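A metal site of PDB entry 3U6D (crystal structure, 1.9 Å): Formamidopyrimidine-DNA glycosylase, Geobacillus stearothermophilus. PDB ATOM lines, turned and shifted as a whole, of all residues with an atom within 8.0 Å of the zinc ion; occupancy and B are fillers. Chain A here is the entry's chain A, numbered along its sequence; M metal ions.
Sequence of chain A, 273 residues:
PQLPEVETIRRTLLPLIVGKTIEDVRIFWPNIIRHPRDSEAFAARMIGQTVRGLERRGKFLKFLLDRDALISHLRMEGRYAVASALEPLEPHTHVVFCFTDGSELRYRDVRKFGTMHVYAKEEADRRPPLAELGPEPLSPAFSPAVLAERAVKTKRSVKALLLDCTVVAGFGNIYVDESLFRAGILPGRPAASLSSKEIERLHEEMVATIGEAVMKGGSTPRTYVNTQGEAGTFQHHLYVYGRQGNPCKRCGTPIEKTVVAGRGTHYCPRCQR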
ATOM      1  N   PHE A 181      28.345   9.253  25.178  1.00  0.00           N
ATOM      2  CA  PHE A 181      27.970   8.226  26.150  1.00  0.00           C
ATOM      3  C   PHE A 181      27.652   8.855  27.503  1.00  0.00           C
ATOM      4  O   PHE A 181      26.635   8.546  28.113  1.00  0.00           O
ATOM      5  CB  PHE A 181      29.063   7.187  26.341  1.00  0.00           C
ATOM      6  CG  PHE A 181      28.810   6.283  27.522  1.00  0.00           C
ATOM      7  CD1 PHE A 181      28.016   5.158  27.391  1.00  0.00           C
ATOM      8  CD2 PHE A 181      29.333   6.594  28.768  1.00  0.00           C
ATOM      9  CE1 PHE A 181      27.764   4.341  28.483  1.00  0.00           C
ATOM     10  CE2 PHE A 181      29.095   5.772  29.859  1.00  0.00           C
ATOM     11  CZ  PHE A 181      28.304   4.659  29.716  1.00  0.00           C
ATOM     12  N   TYR A 239      34.757   4.673  28.435  1.00  0.00           N
ATOM     13  CA  TYR A 239      33.485   3.981  28.612  1.00  0.00           C
ATOM     14  C   TYR A 239      33.097   3.182  27.379  1.00  0.00           C
ATOM     15  O   TYR A 239      32.515   2.104  27.487  1.00  0.00           O
ATOM     16  CB  TYR A 239      32.369   4.969  28.933  1.00  0.00           C
ATOM     17  CG  TYR A 239      32.444   5.562  30.320  1.00  0.00           C
ATOM     18  CD1 TYR A 239      32.918   6.847  30.517  1.00  0.00           C
ATOM     19  CD2 TYR A 239      32.039   4.837  31.429  1.00  0.00           C
ATOM     20  CE1 TYR A 239      32.989   7.402  31.786  1.00  0.00           C
ATOM     21  CE2 TYR A 239      32.109   5.370  32.701  1.00  0.00           C
ATOM     22  CZ  TYR A 239      32.583   6.661  32.870  1.00  0.00           C
ATOM     23  OH  TYR A 239      32.653   7.194  34.142  1.00  0.00           O
ATOM     24  N   VAL A 240      33.404   3.711  26.196  1.00  0.00           N
ATOM     25  CA  VAL A 240      32.937   3.063  24.972  1.00  0.00           C
ATOM     26  C   VAL A 240      33.978   2.925  23.857  1.00  0.00           C
ATOM     27  O   VAL A 240      33.996   1.920  23.148  1.00  0.00           O
ATOM     28  CB  VAL A 240      31.673   3.759  24.414  1.00  0.00           C
ATOM     29  CG1 VAL A 240      30.521   3.680  25.422  1.00  0.00           C
ATOM     30  CG2 VAL A 240      31.966   5.213  24.044  1.00  0.00           C
ATOM     31  N   PRO A 247      31.388  -5.328  28.091  1.00  0.00           N
ATOM     32  CA  PRO A 247      30.283  -4.830  28.900  1.00  0.00           C
ATOM     33  C   PRO A 247      30.396  -3.339  29.175  1.00  0.00           C
ATOM     34  O   PRO A 247      31.485  -2.855  29.512  1.00  0.00           O
ATOM     35  CB  PRO A 247      30.422  -5.603  30.212  1.00  0.00           C
ATOM     36  CG  PRO A 247      31.258  -6.804  29.876  1.00  0.00           C
ATOM     37  CD  PRO A 247      32.197  -6.328  28.813  1.00  0.00           C
ATOM     38  N   CYS A 248      29.294  -2.614  29.027  1.00  0.00           N
ATOM     39  CA  CYS A 248      29.231  -1.233  29.469  1.00  0.00           C
ATOM     40  C   CYS A 248      29.579  -1.169  30.951  1.00  0.00           C
ATOM     41  O   CYS A 248      29.128  -2.003  31.745  1.00  0.00           O
ATOM     42  CB  CYS A 248      27.831  -0.668  29.246  1.00  0.00           C
ATOM     43  SG  CYS A 248      27.617   0.990  29.908  1.00  0.00           S
ATOM     44  N   LYS A 249      30.386  -0.183  31.332  1.00  0.00           N
ATOM     45  CA  LYS A 249      30.827  -0.046  32.714  1.00  0.00           C
ATOM     46  C   LYS A 249      29.729   0.480  33.630  1.00  0.00           C
ATOM     47  O   LYS A 249      29.856   0.418  34.848  1.00  0.00           O
ATOM     48  CB  LYS A 249      32.053   0.873  32.787  1.00  0.00           C
ATOM     49  CG  LYS A 249      33.259   0.319  32.043  1.00  0.00           C
ATOM     50  CD  LYS A 249      34.449   1.265  32.109  1.00  0.00           C
ATOM     51  CE  LYS A 249      35.696   0.613  31.530  1.00  0.00           C
ATOM     52  NZ  LYS A 249      36.874   1.509  31.592  1.00  0.00           N
ATOM     53  N   ARG A 250      28.638   0.980  33.044  1.00  0.00           N
ATOM     54  CA  ARG A 250      27.533   1.529  33.821  1.00  0.00           C
ATOM     55  C   ARG A 250      26.331   0.588  33.902  1.00  0.00           C
ATOM     56  O   ARG A 250      25.615   0.576  34.902  1.00  0.00           O
ATOM     57  CB  ARG A 250      27.101   2.892  33.257  1.00  0.00           C
ATOM     58  CG  ARG A 250      28.142   4.002  33.401  1.00  0.00           C
ATOM     59  CD  ARG A 250      27.848   4.898  34.598  1.00  0.00           C
ATOM     60  NE  ARG A 250      28.797   5.999  34.706  1.00  0.00           N
ATOM     61  CZ  ARG A 250      28.670   7.163  34.081  1.00  0.00           C
ATOM     62  NH1 ARG A 250      27.634   7.389  33.284  1.00  0.00           N
ATOM     63  NH2 ARG A 250      29.590   8.108  34.247  1.00  0.00           N
ATOM     64  N   CYS A 251      26.099  -0.194  32.852  1.00  0.00           N
ATOM     65  CA  CYS A 251      24.928  -1.079  32.821  1.00  0.00           C
ATOM     66  C   CYS A 251      25.190  -2.529  32.424  1.00  0.00           C
ATOM     67  O   CYS A 251      24.295  -3.373  32.543  1.00  0.00           O
ATOM     68  CB  CYS A 251      23.854  -0.483  31.923  1.00  0.00           C
ATOM     69  SG  CYS A 251      24.183  -0.727  30.166  1.00  0.00           S
ATOM     70  N   GLY A 252      26.388  -2.820  31.946  1.00  0.00           N
ATOM     71  CA  GLY A 252      26.754  -4.193  31.601  1.00  0.00           C
ATOM     72  C   GLY A 252      26.349  -4.651  30.209  1.00  0.00           C
ATOM     73  O   GLY A 252      26.722  -5.740  29.771  1.00  0.00           O
ATOM     74  N   THR A 253      25.585  -3.817  29.506  1.00  0.00           N
ATOM     75  CA  THR A 253      25.189  -4.117  28.129  1.00  0.00           C
ATOM     76  C   THR A 253      26.415  -4.067  27.214  1.00  0.00           C
ATOM     77  O   THR A 253      27.232  -3.158  27.337  1.00  0.00           O
ATOM     78  CB  THR A 253      24.163  -3.087  27.615  1.00  0.00           C
ATOM     79  OG1 THR A 253      23.025  -3.053  28.490  1.00  0.00           O
ATOM     80  CG2 THR A 253      23.728  -3.416  26.196  1.00  0.00           C
ATOM     81  N   PRO A 254      26.551  -5.040  26.300  1.00  0.00           N
ATOM     82  CA  PRO A 254      27.717  -5.014  25.402  1.00  0.00           C
ATOM     83  C   PRO A 254      27.789  -3.731  24.576  1.00  0.00           C
ATOM     84  O   PRO A 254      26.797  -3.325  23.980  1.00  0.00           O
ATOM     85  CB  PRO A 254      27.482  -6.220  24.477  1.00  0.00           C
ATOM     86  CG  PRO A 254      26.591  -7.131  25.278  1.00  0.00           C
ATOM     87  CD  PRO A 254      25.689  -6.210  26.050  1.00  0.00           C
ATOM     88  N   ILE A 255      28.952  -3.107  24.552  1.00  0.00           N
ATOM     89  CA  ILE A 255      29.173  -1.928  23.720  1.00  0.00           C
ATOM     90  C   ILE A 255      29.138  -2.357  22.269  1.00  0.00           C
ATOM     91  O   ILE A 255      29.596  -3.446  21.916  1.00  0.00           O
ATOM     92  CB  ILE A 255      30.513  -1.249  24.062  1.00  0.00           C
ATOM     93  CG1 ILE A 255      30.500  -0.790  25.521  1.00  0.00           C
ATOM     94  CG2 ILE A 255      30.758  -0.057  23.130  1.00  0.00           C
ATOM     95  CD1 ILE A 255      29.256   0.031  25.885  1.00  0.00           C
ATOM     96  N   TYR A 267      29.150   2.940  21.158  1.00  0.00           N
ATOM     97  CA  TYR A 267      28.065   3.398  22.015  1.00  0.00           C
ATOM     98  C   TYR A 267      27.437   2.240  22.802  1.00  0.00           C
ATOM     99  O   TYR A 267      27.582   1.070  22.445  1.00  0.00           O
ATOM    100  CB  TYR A 267      26.996   4.089  21.175  1.00  0.00           C
ATOM    101  CG  TYR A 267      26.353   3.153  20.177  1.00  0.00           C
ATOM    102  CD1 TYR A 267      25.159   2.492  20.469  1.00  0.00           C
ATOM    103  CD2 TYR A 267      26.963   2.896  18.949  1.00  0.00           C
ATOM    104  CE1 TYR A 267      24.588   1.616  19.563  1.00  0.00           C
ATOM    105  CE2 TYR A 267      26.385   2.024  18.037  1.00  0.00           C
ATOM    106  CZ  TYR A 267      25.203   1.387  18.349  1.00  0.00           C
ATOM    107  OH  TYR A 267      24.625   0.513  17.451  1.00  0.00           O
ATOM    108  N   CYS A 268      26.762   2.589  23.887  1.00  0.00           N
ATOM    109  CA  CYS A 268      25.944   1.630  24.623  1.00  0.00           C
ATOM    110  C   CYS A 268      24.493   1.863  24.251  1.00  0.00           C
ATOM    111  O   CYS A 268      23.961   2.959  24.461  1.00  0.00           O
ATOM    112  CB  CYS A 268      26.127   1.812  26.122  1.00  0.00           C
ATOM    113  SG  CYS A 268      25.002   0.768  27.056  1.00  0.00           S
ATOM    114  N   PRO A 269      23.850   0.841  23.683  1.00  0.00           N
ATOM    115  CA  PRO A 269      22.467   1.001  23.220  1.00  0.00           C
ATOM    116  C   PRO A 269      21.452   1.101  24.362  1.00  0.00           C
ATOM    117  O   PRO A 269      20.286   1.371  24.094  1.00  0.00           O
ATOM    118  CB  PRO A 269      22.226  -0.271  22.403  1.00  0.00           C
ATOM    119  CG  PRO A 269      23.129  -1.271  23.007  1.00  0.00           C
ATOM    120  CD  PRO A 269      24.362  -0.507  23.407  1.00  0.00           C
ATOM    121  N   ARG A 270      21.878   0.879  25.601  1.00  0.00           N
ATOM    122  CA  ARG A 270      20.965   1.048  26.742  1.00  0.00           C
ATOM    123  C   ARG A 270      21.118   2.412  27.408  1.00  0.00           C
ATOM    124  O   ARG A 270      20.120   3.090  27.668  1.00  0.00           O
ATOM    125  CB  ARG A 270      21.149  -0.066  27.777  1.00  0.00           C
ATOM    126  CG  ARG A 270      20.307   0.137  29.027  1.00  0.00           C
ATOM    127  CD  ARG A 270      20.384  -1.042  30.005  1.00  0.00           C
ATOM    128  NE  ARG A 270      19.452  -0.836  31.112  1.00  0.00           N
ATOM    129  CZ  ARG A 270      19.249  -1.695  32.106  1.00  0.00           C
ATOM    130  NH1 ARG A 270      18.358  -1.393  33.053  1.00  0.00           N
ATOM    131  NH2 ARG A 270      19.925  -2.833  32.167  1.00  0.00           N
ATOM    132  N   CYS A 271      22.357   2.802  27.699  1.00  0.00           N
ATOM    133  CA  CYS A 271      22.624   4.093  28.337  1.00  0.00           C
ATOM    134  C   CYS A 271      22.346   5.284  27.424  1.00  0.00           C
ATOM    135  O   CYS A 271      21.987   6.359  27.902  1.00  0.00           O
ATOM    136  CB  CYS A 271      24.076   4.186  28.830  1.00  0.00           C
ATOM    137  SG  CYS A 271      24.475   3.112  30.226  1.00  0.00           S
ATOM    138  N   GLN A 272      22.530   5.108  26.115  1.00  0.00           N
ATOM    139  CA  GLN A 272      22.349   6.219  25.188  1.00  0.00           C
ATOM    140  C   GLN A 272      21.041   6.084  24.428  1.00  0.00           C
ATOM    141  O   GLN A 272      20.696   4.992  23.976  1.00  0.00           O
ATOM    142  CB  GLN A 272      23.528   6.301  24.216  1.00  0.00           C
ATOM    143  CG  GLN A 272      24.845   6.578  24.914  1.00  0.00           C
ATOM    144  CD  GLN A 272      26.054   6.375  24.027  1.00  0.00           C
ATOM    145  OE1 GLN A 272      26.788   5.398  24.197  1.00  0.00           O
ATOM    146  NE2 GLN A 272      26.274   7.299  23.106  1.00  0.00           N
HETATM  147 ZN    ZN M   1      25.305   1.177  29.340  1.00  0.00          ZN
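The backbone NH (N) of Arg 270 lies close to the side-chain sulfur (SG) of Cys 268.
The backbone NH of Cys 268 sits at hydrogen-bond distance from the side-chain amide oxygen of Gln 272 (2.8 Å).
The side-chain hydroxyl (OG1) of Thr 253 lies close to the side-chain sulfur (SG) of Cys 251, 3.1 Å away.
SG of Cys 248 sits close to N of Arg 250 (3.3 Å).
O of Thr 253 is in hydrogen-bond range of N of Cys 248, 2.7 Å away.
Of the 18 residues printed, 4 come within 4 Å of the zinc ion.
The nearest printed residue that does not touch the zinc ion is Phe 181 (4.1 Å).
The zinc ion is bound by SG of Cys 271 (2.3 Å), SG of Cys 268 (2.3 Å), SG of Cys 251 (2.4 Å) and SG of Cys 248 (2.4 Å).
The zinc ion has four donor atoms within binding distance.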
